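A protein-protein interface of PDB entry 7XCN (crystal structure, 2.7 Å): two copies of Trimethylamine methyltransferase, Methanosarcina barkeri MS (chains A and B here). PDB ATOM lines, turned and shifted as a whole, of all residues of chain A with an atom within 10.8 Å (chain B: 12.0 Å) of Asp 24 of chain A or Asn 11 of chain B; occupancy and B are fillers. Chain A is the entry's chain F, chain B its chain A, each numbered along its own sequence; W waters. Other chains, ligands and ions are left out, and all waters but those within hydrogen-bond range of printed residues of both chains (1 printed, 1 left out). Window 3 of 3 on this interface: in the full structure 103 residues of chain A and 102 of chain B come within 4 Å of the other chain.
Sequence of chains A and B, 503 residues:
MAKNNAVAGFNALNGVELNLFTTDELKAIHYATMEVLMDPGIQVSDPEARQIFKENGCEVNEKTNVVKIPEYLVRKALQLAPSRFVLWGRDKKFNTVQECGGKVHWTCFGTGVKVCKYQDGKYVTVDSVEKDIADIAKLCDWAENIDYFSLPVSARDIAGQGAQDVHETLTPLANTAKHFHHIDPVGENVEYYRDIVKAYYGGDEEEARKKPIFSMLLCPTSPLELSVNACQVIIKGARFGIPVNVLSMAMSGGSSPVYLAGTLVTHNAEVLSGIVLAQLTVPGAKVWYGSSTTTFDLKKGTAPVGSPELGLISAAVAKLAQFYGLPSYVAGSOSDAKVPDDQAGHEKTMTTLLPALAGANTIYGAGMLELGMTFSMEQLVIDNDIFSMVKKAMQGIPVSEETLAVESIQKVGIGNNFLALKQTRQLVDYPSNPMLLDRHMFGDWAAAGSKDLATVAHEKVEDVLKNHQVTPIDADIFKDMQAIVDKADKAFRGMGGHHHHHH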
ATOM      1  N   LEU A  20      18.718 -26.536  -6.536  1.00  0.00           N
ATOM      2  CA  LEU A  20      17.997 -25.492  -5.817  1.00  0.00           C
ATOM      3  C   LEU A  20      18.202 -24.123  -6.458  1.00  0.00           C
ATOM      4  O   LEU A  20      17.379 -23.221  -6.316  1.00  0.00           O
ATOM      5  CB  LEU A  20      18.478 -25.426  -4.367  1.00  0.00           C
ATOM      6  CG  LEU A  20      18.053 -26.568  -3.451  1.00  0.00           C
ATOM      7  CD1 LEU A  20      18.671 -26.345  -2.085  1.00  0.00           C
ATOM      8  CD2 LEU A  20      16.536 -26.630  -3.354  1.00  0.00           C
ATOM      9  N   PHE A  21      19.299 -23.979  -7.181  1.00  0.00           N
ATOM     10  CA  PHE A  21      19.615 -22.703  -7.786  1.00  0.00           C
ATOM     11  C   PHE A  21      20.147 -22.755  -9.203  1.00  0.00           C
ATOM     12  O   PHE A  21      20.530 -23.802  -9.720  1.00  0.00           O
ATOM     13  CB  PHE A  21      20.675 -21.987  -6.950  1.00  0.00           C
ATOM     14  CG  PHE A  21      20.334 -21.863  -5.502  1.00  0.00           C
ATOM     15  CD1 PHE A  21      19.279 -21.061  -5.084  1.00  0.00           C
ATOM     16  CD2 PHE A  21      21.102 -22.509  -4.547  1.00  0.00           C
ATOM     17  CE1 PHE A  21      19.000 -20.903  -3.735  1.00  0.00           C
ATOM     18  CE2 PHE A  21      20.834 -22.358  -3.201  1.00  0.00           C
ATOM     19  CZ  PHE A  21      19.782 -21.553  -2.790  1.00  0.00           C
ATOM     20  N   THR A  22      20.178 -21.578  -9.807  1.00  0.00           N
ATOM     21  CA  THR A  22      20.734 -21.382 -11.132  1.00  0.00           C
ATOM     22  C   THR A  22      21.925 -20.486 -10.816  1.00  0.00           C
ATOM     23  O   THR A  22      22.001 -19.913  -9.724  1.00  0.00           O
ATOM     24  CB  THR A  22      19.786 -20.607 -12.060  1.00  0.00           C
ATOM     25  OG1 THR A  22      19.601 -19.279 -11.551  1.00  0.00           O
ATOM     26  CG2 THR A  22      18.455 -21.307 -12.155  1.00  0.00           C
ATOM     27  N   THR A  23      22.850 -20.362 -11.755  1.00  0.00           N
ATOM     28  CA  THR A  23      24.005 -19.525 -11.524  1.00  0.00           C
ATOM     29  C   THR A  23      23.560 -18.118 -11.151  1.00  0.00           C
ATOM     30  O   THR A  23      24.079 -17.533 -10.211  1.00  0.00           O
ATOM     31  CB  THR A  23      24.880 -19.473 -12.758  1.00  0.00           C
ATOM     32  OG1 THR A  23      25.271 -20.807 -13.100  1.00  0.00           O
ATOM     33  CG2 THR A  23      26.122 -18.635 -12.488  1.00  0.00           C
ATOM     34  N   ASP A  24      22.588 -17.585 -11.881  1.00  0.00           N
ATOM     35  CA  ASP A  24      22.079 -16.249 -11.606  1.00  0.00           C
ATOM     36  C   ASP A  24      21.659 -16.091 -10.157  1.00  0.00           C
ATOM     37  O   ASP A  24      21.906 -15.052  -9.544  1.00  0.00           O
ATOM     38  CB  ASP A  24      20.879 -15.926 -12.496  1.00  0.00           C
ATOM     39  CG  ASP A  24      21.268 -15.682 -13.943  1.00  0.00           C
ATOM     40  OD1 ASP A  24      22.340 -15.074 -14.184  1.00  0.00           O
ATOM     41  OD2 ASP A  24      20.493 -16.082 -14.842  1.00  0.00           O
ATOM     42  N   GLU A  25      21.018 -17.121  -9.612  1.00  0.00           N
ATOM     43  CA  GLU A  25      20.565 -17.071  -8.231  1.00  0.00           C
ATOM     44  C   GLU A  25      21.719 -17.122  -7.239  1.00  0.00           C
ATOM     45  O   GLU A  25      21.710 -16.393  -6.255  1.00  0.00           O
ATOM     46  CB  GLU A  25      19.559 -18.193  -7.971  1.00  0.00           C
ATOM     47  CG  GLU A  25      18.270 -18.010  -8.771  1.00  0.00           C
ATOM     48  CD  GLU A  25      17.299 -19.168  -8.635  1.00  0.00           C
ATOM     49  OE1 GLU A  25      17.696 -20.319  -8.927  1.00  0.00           O
ATOM     50  OE2 GLU A  25      16.135 -18.919  -8.245  1.00  0.00           O
ATOM     51  N   LEU A  26      22.715 -17.965  -7.491  1.00  0.00           N
ATOM     52  CA  LEU A  26      23.848 -18.033  -6.580  1.00  0.00           C
ATOM     53  C   LEU A  26      24.546 -16.668  -6.583  1.00  0.00           C
ATOM     54  O   LEU A  26      24.997 -16.185  -5.547  1.00  0.00           O
ATOM     55  CB  LEU A  26      24.824 -19.142  -6.993  1.00  0.00           C
ATOM     56  CG  LEU A  26      24.320 -20.573  -6.819  1.00  0.00           C
ATOM     57  CD1 LEU A  26      25.373 -21.561  -7.303  1.00  0.00           C
ATOM     58  CD2 LEU A  26      24.000 -20.814  -5.356  1.00  0.00           C
ATOM     59  N   LYS A  27      24.619 -16.046  -7.754  1.00  0.00           N
ATOM     60  CA  LYS A  27      25.236 -14.733  -7.886  1.00  0.00           C
ATOM     61  C   LYS A  27      24.454 -13.712  -7.071  1.00  0.00           C
ATOM     62  O   LYS A  27      25.035 -12.855  -6.409  1.00  0.00           O
ATOM     63  CB  LYS A  27      25.242 -14.290  -9.345  1.00  0.00           C
ATOM     64  CG  LYS A  27      26.079 -15.156 -10.252  1.00  0.00           C
ATOM     65  CD  LYS A  27      27.532 -14.739 -10.244  1.00  0.00           C
ATOM     66  CE  LYS A  27      28.273 -15.411 -11.385  1.00  0.00           C
ATOM     67  NZ  LYS A  27      27.566 -15.176 -12.684  1.00  0.00           N
ATOM     68  N   ALA A  28      23.132 -13.807  -7.131  1.00  0.00           N
ATOM     69  CA  ALA A  28      22.265 -12.901  -6.390  1.00  0.00           C
ATOM     70  C   ALA A  28      22.597 -12.941  -4.896  1.00  0.00           C
ATOM     71  O   ALA A  28      22.732 -11.900  -4.255  1.00  0.00           O
ATOM     72  CB  ALA A  28      20.775 -13.270  -6.623  1.00  0.00           C
ATOM     73  N   ILE A  29      22.723 -14.146  -4.354  1.00  0.00           N
ATOM     74  CA  ILE A  29      23.024 -14.340  -2.945  1.00  0.00           C
ATOM     75  C   ILE A  29      24.424 -13.814  -2.634  1.00  0.00           C
ATOM     76  O   ILE A  29      24.662 -13.232  -1.572  1.00  0.00           O
ATOM     77  CB  ILE A  29      22.921 -15.828  -2.587  1.00  0.00           C
ATOM     78  CG1 ILE A  29      21.474 -16.296  -2.788  1.00  0.00           C
ATOM     79  CG2 ILE A  29      23.402 -16.069  -1.155  1.00  0.00           C
ATOM     80  CD1 ILE A  29      21.285 -17.793  -2.601  1.00  0.00           C
ATOM     81  N   HIS A  30      25.346 -14.008  -3.572  1.00  0.00           N
ATOM     82  CA  HIS A  30      26.711 -13.543  -3.395  1.00  0.00           C
ATOM     83  C   HIS A  30      26.764 -12.020  -3.347  1.00  0.00           C
ATOM     84  O   HIS A  30      27.385 -11.445  -2.464  1.00  0.00           O
ATOM     85  CB  HIS A  30      27.596 -14.029  -4.532  1.00  0.00           C
ATOM     86  CG  HIS A  30      29.008 -13.542  -4.433  1.00  0.00           C
ATOM     87  ND1 HIS A  30      29.860 -13.940  -3.427  1.00  0.00           N
ATOM     88  CD2 HIS A  30      29.707 -12.665  -5.192  1.00  0.00           C
ATOM     89  CE1 HIS A  30      31.022 -13.329  -3.570  1.00  0.00           C
ATOM     90  NE2 HIS A  30      30.954 -12.551  -4.635  1.00  0.00           N
ATOM     91  N   TYR A  31      26.125 -11.366  -4.308  1.00  0.00           N
ATOM     92  CA  TYR A  31      26.112  -9.909  -4.336  1.00  0.00           C
ATOM     93  C   TYR A  31      25.450  -9.373  -3.075  1.00  0.00           C
ATOM     94  O   TYR A  31      25.936  -8.428  -2.460  1.00  0.00           O
ATOM     95  CB  TYR A  31      25.362  -9.388  -5.557  1.00  0.00           C
ATOM     96  CG  TYR A  31      25.980  -9.768  -6.871  1.00  0.00           C
ATOM     97  CD1 TYR A  31      27.359  -9.786  -7.029  1.00  0.00           C
ATOM     98  CD2 TYR A  31      25.185 -10.094  -7.971  1.00  0.00           C
ATOM     99  CE1 TYR A  31      27.937 -10.123  -8.250  1.00  0.00           C
ATOM    100  CE2 TYR A  31      25.753 -10.428  -9.196  1.00  0.00           C
ATOM    101  CZ  TYR A  31      27.127 -10.440  -9.325  1.00  0.00           C
ATOM    102  OH  TYR A  31      27.691 -10.767 -10.533  1.00  0.00           O
ATOM    103  N   ALA A  32      24.340  -9.984  -2.686  1.00  0.00           N
ATOM    104  CA  ALA A  32      23.640  -9.563  -1.488  1.00  0.00           C
ATOM    105  C   ALA A  32      24.564  -9.678  -0.277  1.00  0.00           C
ATOM    106  O   ALA A  32      24.517  -8.852   0.624  1.00  0.00           O
ATOM    107  CB  ALA A  32      22.399 -10.410  -1.290  1.00  0.00           C
ATOM    108  N   ALA A 261      16.224 -17.358   1.685  1.00  0.00           N
ATOM    109  CA  ALA A 261      17.293 -16.731   0.917  1.00  0.00           C
ATOM    110  C   ALA A 261      17.998 -15.646   1.737  1.00  0.00           C
ATOM    111  O   ALA A 261      19.222 -15.601   1.789  1.00  0.00           O
ATOM    112  CB  ALA A 261      16.733 -16.134  -0.366  1.00  0.00           C
ATOM    113  N   LEU A 320      26.164 -23.797  -1.931  1.00  0.00           N
ATOM    114  CA  LEU A 320      26.946 -22.571  -1.805  1.00  0.00           C
ATOM    115  C   LEU A 320      28.418 -22.893  -1.604  1.00  0.00           C
ATOM    116  O   LEU A 320      29.290 -22.255  -2.189  1.00  0.00           O
ATOM    117  CB  LEU A 320      26.451 -21.740  -0.629  1.00  0.00           C
ATOM    118  CG  LEU A 320      25.283 -20.821  -0.955  1.00  0.00           C
ATOM    119  CD1 LEU A 320      24.663 -20.309   0.334  1.00  0.00           C
ATOM    120  CD2 LEU A 320      25.782 -19.685  -1.824  1.00  0.00           C
ATOM    121  N   PHE A 323      29.729 -23.809  -4.793  1.00  0.00           N
ATOM    122  CA  PHE A 323      29.859 -22.597  -5.580  1.00  0.00           C
ATOM    123  C   PHE A 323      31.129 -21.829  -5.243  1.00  0.00           C
ATOM    124  O   PHE A 323      31.788 -21.324  -6.132  1.00  0.00           O
ATOM    125  CB  PHE A 323      28.648 -21.708  -5.335  1.00  0.00           C
ATOM    126  CG  PHE A 323      28.730 -20.366  -5.994  1.00  0.00           C
ATOM    127  CD1 PHE A 323      28.697 -20.250  -7.377  1.00  0.00           C
ATOM    128  CD2 PHE A 323      28.765 -19.209  -5.222  1.00  0.00           C
ATOM    129  CE1 PHE A 323      28.685 -18.994  -7.989  1.00  0.00           C
ATOM    130  CE2 PHE A 323      28.756 -17.953  -5.819  1.00  0.00           C
ATOM    131  CZ  PHE A 323      28.712 -17.844  -7.212  1.00  0.00           C
ATOM    132  N   TYR A 324      31.460 -21.739  -3.960  1.00  0.00           N
ATOM    133  CA  TYR A 324      32.649 -21.022  -3.529  1.00  0.00           C
ATOM    134  C   TYR A 324      33.903 -21.886  -3.561  1.00  0.00           C
ATOM    135  O   TYR A 324      35.000 -21.397  -3.317  1.00  0.00           O
ATOM    136  CB  TYR A 324      32.451 -20.447  -2.124  1.00  0.00           C
ATOM    137  CG  TYR A 324      31.513 -19.266  -2.077  1.00  0.00           C
ATOM    138  CD1 TYR A 324      31.665 -18.200  -2.963  1.00  0.00           C
ATOM    139  CD2 TYR A 324      30.500 -19.185  -1.118  1.00  0.00           C
ATOM    140  CE1 TYR A 324      30.838 -17.079  -2.896  1.00  0.00           C
ATOM    141  CE2 TYR A 324      29.662 -18.066  -1.040  1.00  0.00           C
ATOM    142  CZ  TYR A 324      29.841 -17.017  -1.932  1.00  0.00           C
ATOM    143  OH  TYR A 324      29.028 -15.904  -1.863  1.00  0.00           O
ATOM    144  N   VAL B   7      15.115  -5.238 -14.419  1.00  0.00           N
ATOM    145  CA  VAL B   7      16.216  -6.173 -14.512  1.00  0.00           C
ATOM    146  C   VAL B   7      16.087  -6.839 -15.863  1.00  0.00           C
ATOM    147  O   VAL B   7      14.986  -6.934 -16.401  1.00  0.00           O
ATOM    148  CB  VAL B   7      16.105  -7.245 -13.440  1.00  0.00           C
ATOM    149  CG1 VAL B   7      17.307  -8.179 -13.508  1.00  0.00           C
ATOM    150  CG2 VAL B   7      15.981  -6.592 -12.083  1.00  0.00           C
ATOM    151  N   ALA B   8      17.201  -7.303 -16.415  1.00  0.00           N
ATOM    152  CA  ALA B   8      17.152  -7.948 -17.714  1.00  0.00           C
ATOM    153  C   ALA B   8      16.975  -9.428 -17.530  1.00  0.00           C
ATOM    154  O   ALA B   8      16.740  -9.887 -16.425  1.00  0.00           O
ATOM    155  CB  ALA B   8      18.413  -7.674 -18.487  1.00  0.00           C
ATOM    156  N   GLY B   9      17.104 -10.168 -18.626  1.00  0.00           N
ATOM    157  CA  GLY B   9      16.955 -11.615 -18.594  1.00  0.00           C
ATOM    158  C   GLY B   9      17.599 -12.301 -17.408  1.00  0.00           C
ATOM    159  O   GLY B   9      18.805 -12.206 -17.222  1.00  0.00           O
ATOM    160  N   PHE B  10      16.778 -13.007 -16.628  1.00  0.00           N
ATOM    161  CA  PHE B  10      17.220 -13.723 -15.424  1.00  0.00           C
ATOM    162  C   PHE B  10      16.674 -15.165 -15.398  1.00  0.00           C
ATOM    163  O   PHE B  10      15.487 -15.389 -15.621  1.00  0.00           O
ATOM    164  CB  PHE B  10      16.728 -12.959 -14.195  1.00  0.00           C
ATOM    165  CG  PHE B  10      17.206 -13.513 -12.890  1.00  0.00           C
ATOM    166  CD1 PHE B  10      18.494 -13.251 -12.436  1.00  0.00           C
ATOM    167  CD2 PHE B  10      16.352 -14.257 -12.085  1.00  0.00           C
ATOM    168  CE1 PHE B  10      18.928 -13.720 -11.186  1.00  0.00           C
ATOM    169  CE2 PHE B  10      16.774 -14.732 -10.838  1.00  0.00           C
ATOM    170  CZ  PHE B  10      18.066 -14.460 -10.390  1.00  0.00           C
ATOM    171  N   ASN B  11      17.537 -16.140 -15.126  1.00  0.00           N
ATOM    172  CA  ASN B  11      17.104 -17.532 -15.075  1.00  0.00           C
ATOM    173  C   ASN B  11      16.944 -18.015 -13.654  1.00  0.00           C
ATOM    174  O   ASN B  11      17.854 -17.903 -12.835  1.00  0.00           O
ATOM    175  CB  ASN B  11      18.074 -18.427 -15.820  1.00  0.00           C
ATOM    176  CG  ASN B  11      17.967 -18.259 -17.321  1.00  0.00           C
ATOM    177  OD1 ASN B  11      18.692 -17.468 -17.924  1.00  0.00           O
ATOM    178  ND2 ASN B  11      17.038 -18.990 -17.932  1.00  0.00           N
ATOM    179  N   ALA B  12      15.776 -18.564 -13.360  1.00  0.00           N
ATOM    180  CA  ALA B  12      15.492 -19.021 -12.017  1.00  0.00           C
ATOM    181  C   ALA B  12      15.009 -20.451 -11.974  1.00  0.00           C
ATOM    182  O   ALA B  12      14.502 -20.975 -12.962  1.00  0.00           O
ATOM    183  CB  ALA B  12      14.448 -18.112 -11.384  1.00  0.00           C
ATOM    184  N   LEU B  13      15.184 -21.077 -10.815  1.00  0.00           N
ATOM    185  CA  LEU B  13      14.721 -22.430 -10.605  1.00  0.00           C
ATOM    186  C   LEU B  13      13.677 -22.342  -9.506  1.00  0.00           C
ATOM    187  O   LEU B  13      13.972 -21.955  -8.369  1.00  0.00           O
ATOM    188  CB  LEU B  13      15.860 -23.364 -10.186  1.00  0.00           C
ATOM    189  CG  LEU B  13      15.384 -24.777  -9.817  1.00  0.00           C
ATOM    190  CD1 LEU B  13      16.171 -25.790 -10.600  1.00  0.00           C
ATOM    191  CD2 LEU B  13      15.534 -25.013  -8.322  1.00  0.00           C
ATOM    192  N   ASN B  14      12.448 -22.684  -9.861  1.00  0.00           N
ATOM    193  CA  ASN B  14      11.358 -22.637  -8.918  1.00  0.00           C
ATOM    194  C   ASN B  14      11.120 -23.971  -8.245  1.00  0.00           C
ATOM    195  O   ASN B  14      10.626 -24.927  -8.861  1.00  0.00           O
ATOM    196  CB  ASN B  14      10.086 -22.152  -9.612  1.00  0.00           C
ATOM    197  CG  ASN B  14      10.222 -20.733 -10.126  1.00  0.00           C
ATOM    198  OD1 ASN B  14      10.933 -19.922  -9.531  1.00  0.00           O
ATOM    199  ND2 ASN B  14       9.535 -20.421 -11.223  1.00  0.00           N
ATOM    200  N   GLY B  15      11.475 -24.021  -6.966  1.00  0.00           N
ATOM    201  CA  GLY B  15      11.299 -25.235  -6.203  1.00  0.00           C
ATOM    202  C   GLY B  15      12.584 -26.018  -6.093  1.00  0.00           C
ATOM    203  O   GLY B  15      13.647 -25.454  -5.882  1.00  0.00           O
ATOM    204  N   GLU B  17      14.621 -29.155  -8.149  1.00  0.00           N
ATOM    205  CA  GLU B  17      14.610 -30.094  -9.248  1.00  0.00           C
ATOM    206  C   GLU B  17      15.463 -31.301  -8.880  1.00  0.00           C
ATOM    207  O   GLU B  17      16.545 -31.167  -8.300  1.00  0.00           O
ATOM    208  CB  GLU B  17      15.119 -29.423 -10.524  1.00  0.00           C
ATOM    209  CG  GLU B  17      15.285 -30.369 -11.689  1.00  0.00           C
ATOM    210  CD  GLU B  17      15.645 -29.647 -12.971  1.00  0.00           C
ATOM    211  OE1 GLU B  17      16.400 -28.651 -12.898  1.00  0.00           O
ATOM    212  OE2 GLU B  17      15.184 -30.087 -14.051  1.00  0.00           O
ATOM    213  N   ILE B 397      14.052 -22.795  -2.366  1.00  0.00           N
ATOM    214  CA  ILE B 397      14.471 -21.522  -1.801  1.00  0.00           C
ATOM    215  C   ILE B 397      14.254 -20.404  -2.824  1.00  0.00           C
ATOM    216  O   ILE B 397      15.064 -20.192  -3.726  1.00  0.00           O
ATOM    217  CB  ILE B 397      15.958 -21.591  -1.392  1.00  0.00           C
ATOM    218  CG1 ILE B 397      16.093 -22.430  -0.128  1.00  0.00           C
ATOM    219  CG2 ILE B 397      16.516 -20.207  -1.179  1.00  0.00           C
ATOM    220  CD1 ILE B 397      17.490 -22.764   0.226  1.00  0.00           C
ATOM    221  N   PRO B 398      13.133 -19.685  -2.713  1.00  0.00           N
ATOM    222  CA  PRO B 398      12.867 -18.597  -3.662  1.00  0.00           C
ATOM    223  C   PRO B 398      13.917 -17.499  -3.519  1.00  0.00           C
ATOM    224  O   PRO B 398      14.199 -17.035  -2.404  1.00  0.00           O
ATOM    225  CB  PRO B 398      11.485 -18.115  -3.252  1.00  0.00           C
ATOM    226  CG  PRO B 398      10.868 -19.326  -2.653  1.00  0.00           C
ATOM    227  CD  PRO B 398      11.975 -19.915  -1.836  1.00  0.00           C
ATOM    228  N   VAL B 399      14.506 -17.100  -4.640  1.00  0.00           N
ATOM    229  CA  VAL B 399      15.519 -16.052  -4.617  1.00  0.00           C
ATOM    230  C   VAL B 399      15.063 -14.870  -5.451  1.00  0.00           C
ATOM    231  O   VAL B 399      15.001 -14.956  -6.677  1.00  0.00           O
ATOM    232  CB  VAL B 399      16.887 -16.527  -5.186  1.00  0.00           C
ATOM    233  CG1 VAL B 399      17.884 -15.402  -5.114  1.00  0.00           C
ATOM    234  CG2 VAL B 399      17.418 -17.705  -4.403  1.00  0.00           C
ATOM    235  N   SER B 400      14.729 -13.778  -4.769  1.00  0.00           N
ATOM    236  CA  SER B 400      14.307 -12.530  -5.406  1.00  0.00           C
ATOM    237  C   SER B 400      14.944 -11.433  -4.570  1.00  0.00           C
ATOM    238  O   SER B 400      15.631 -11.722  -3.586  1.00  0.00           O
ATOM    239  CB  SER B 400      12.782 -12.370  -5.378  1.00  0.00           C
ATOM    240  OG  SER B 400      12.302 -12.148  -4.063  1.00  0.00           O
ATOM    241  N   GLU B 401      14.727 -10.178  -4.942  1.00  0.00           N
ATOM    242  CA  GLU B 401      15.306  -9.100  -4.165  1.00  0.00           C
ATOM    243  C   GLU B 401      14.556  -9.040  -2.846  1.00  0.00           C
ATOM    244  O   GLU B 401      15.135  -8.752  -1.795  1.00  0.00           O
ATOM    245  CB  GLU B 401      15.198  -7.773  -4.918  1.00  0.00           C
ATOM    246  CG  GLU B 401      15.931  -7.771  -6.264  1.00  0.00           C
ATOM    247  CD  GLU B 401      17.412  -8.147  -6.157  1.00  0.00           C
ATOM    248  OE1 GLU B 401      18.170  -7.422  -5.473  1.00  0.00           O
ATOM    249  OE2 GLU B 401      17.816  -9.168  -6.763  1.00  0.00           O
ATOM    250  N   THR B 403      13.141 -11.594  -1.175  1.00  0.00           N
ATOM    251  CA  THR B 403      13.585 -12.671  -0.286  1.00  0.00           C
ATOM    252  C   THR B 403      15.048 -12.602   0.150  1.00  0.00           C
ATOM    253  O   THR B 403      15.382 -13.158   1.190  1.00  0.00           O
ATOM    254  CB  THR B 403      13.319 -14.080  -0.891  1.00  0.00           C
ATOM    255  OG1 THR B 403      13.880 -14.163  -2.205  1.00  0.00           O
ATOM    256  CG2 THR B 403      11.826 -14.353  -0.968  1.00  0.00           C
ATOM    257  N   LEU B 404      15.919 -11.946  -0.630  1.00  0.00           N
ATOM    258  CA  LEU B 404      17.329 -11.832  -0.234  1.00  0.00           C
ATOM    259  C   LEU B 404      17.337 -10.885   0.968  1.00  0.00           C
ATOM    260  O   LEU B 404      18.237 -10.922   1.817  1.00  0.00           O
ATOM    261  CB  LEU B 404      18.189 -11.276  -1.384  1.00  0.00           C
ATOM    262  CG  LEU B 404      18.443 -12.187  -2.599  1.00  0.00           C
ATOM    263  CD1 LEU B 404      18.870 -11.341  -3.765  1.00  0.00           C
ATOM    264  CD2 LEU B 404      19.496 -13.238  -2.291  1.00  0.00           C
HETATM  265  O   HOH W   1      15.149 -23.651  -4.930  1.00  0.00           O
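The side-chain hydroxyl (OG1) of Thr 22 of chain A is in hydrogen-bond range of the backbone carbonyl oxygen (O) of Asn 11 of chain B. N of Asn 11 of chain B sits at hydrogen-bond distance from OD2 of Asp 24 of chain A (3.0 Å). The side-chain carboxylate (OE1) of Glu 25 of chain A sits at hydrogen-bond distance from the backbone NH (N) of Leu 13 of chain B, at 3.2 Å.
Of the 17 printed residues of chain A, 8 touch a printed residue of chain B. Printed residues of chain A that touch a printed residue of chain B: Leu 20, Phe 21, Thr 22, Asp 24, Glu 25, Ala 28, Ile 29 and Ala 261. Hydrophobic or aromatic side chains of chain A that line the printed part of chain B: Phe 21, Ala 28, Ile 29 and Ala 261. Of the 17 printed residues of chain B, 9 touch a printed residue of chain A. Hydrophobic or aromatic side chains of chain B within 4 Å of the printed part of chain A: Phe 10, Ala 12, Leu 13, Ile 397, Val 399 and Leu 404. Along chain B the printed residues that touch a printed residue of chain A span positions 10 to 404. Among the printed residues, no Asp or Glu carboxylate lies within 4 Å of a Lys or Arg side-chain nitrogen of the other chain.
Among the printed residues, pairs that only touch across the chains: Asp 24 of chain A with Phe 10 of chain B (3.2 Å), Leu 20 of chain A with Leu 13 of chain B (3.3 Å), Ala 261 of chain A with Pro 398 of chain B (3.4 Å), Thr 22 of chain A with Leu 13 of chain B (3.5 Å), Thr 22 of chain A with Ala 12 of chain B (3.6 Å), Ala 261 of chain A with Thr 403 of chain B (3.6 Å), Phe 21 of chain A with Val 399 of chain B (3.6 Å), Phe 21 of chain A with Ile 397 of chain B (3.6 Å), Glu 25 of chain A with Ala 12 of chain B (3.7 Å), Ile 29 of chain A with Leu 404 of chain B (3.7 Å), Ala 28 of chain A with Val 399 of chain B (3.9 Å), Glu 25 of chain A with Phe 10 of chain B (3.9 Å), Ala 28 of chain A with Leu 404 of chain B (3.9 Å) and Glu 25 of chain A with Val 399 of chain B (3.96 Å).
OG1 of Thr 403 of chain B sits at hydrogen-bond distance from O of Pro 398 of chain B, 2.9 Å away. OG1 of Thr 403 of chain B is in hydrogen-bond range of N of Ser 400 of chain B, at 2.7 Å. The side-chain hydroxyl (OG1) of Thr 22 of chain A lies close to the backbone NH (N) of Asp 24 of chain A (3.4 Å). The side-chain carboxylate of Glu 25 of chain A lies within hydrogen-bond range of the backbone NH of Thr 22 of chain A, 2.9 Å away.
No position is printed for both chains. Of the 17 pairs that touch across the chains among the printed residues, none has its exchanged pair printed and touching as well.
Of chain B, only Asn 11 (2.6 Å), Ala 12 (3.6 Å) and Leu 13 (3.5 Å) come within 4 Å of Thr 22 of chain A. Asp 24 of chain A touches just these residues of chain B: Phe 10 and Asn 11. Of chain B, only Phe 10 (3.9 Å), Ala 12 (3.7 Å), Leu 13 (3.2 Å) and Val 399 (3.96 Å) come within 4 Å of Glu 25 of chain A. No residue of chain B comes within 4 Å of Leu 26 of chain A. Ala 28 of chain A touches just these residues of chain B: Val 399 and Leu 404. Of chain A, only Thr 22 and Asp 24 come within 4 Å of Asn 11 of chain B. Of the printed residues of chain A, Ala 12 of chain B touches Thr 22 (3.6 Å) and Glu 25 (3.7 Å). Of the printed residues of chain A, Leu 13 of chain B touches Leu 20 (3.3 Å), Thr 22 (3.5 Å) and Glu 25 (3.2 Å). Printed residues of chain A within 4 Å of Val 399 of chain B: Phe 21, Glu 25 and Ala 28. The nearest residue of chain B that does not touch Asp 24 of chain A is Gly 9 of chain B (4.9 Å). The nearest printed residue of chain A that does not touch Thr 403 of chain B is Ala 32 of chain A (7.8 Å).
Water W1 lies within hydrogen-bond range of O of Gly 15 of chain B, O of Leu 20 of chain A and N of Ile 397 of chain B.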
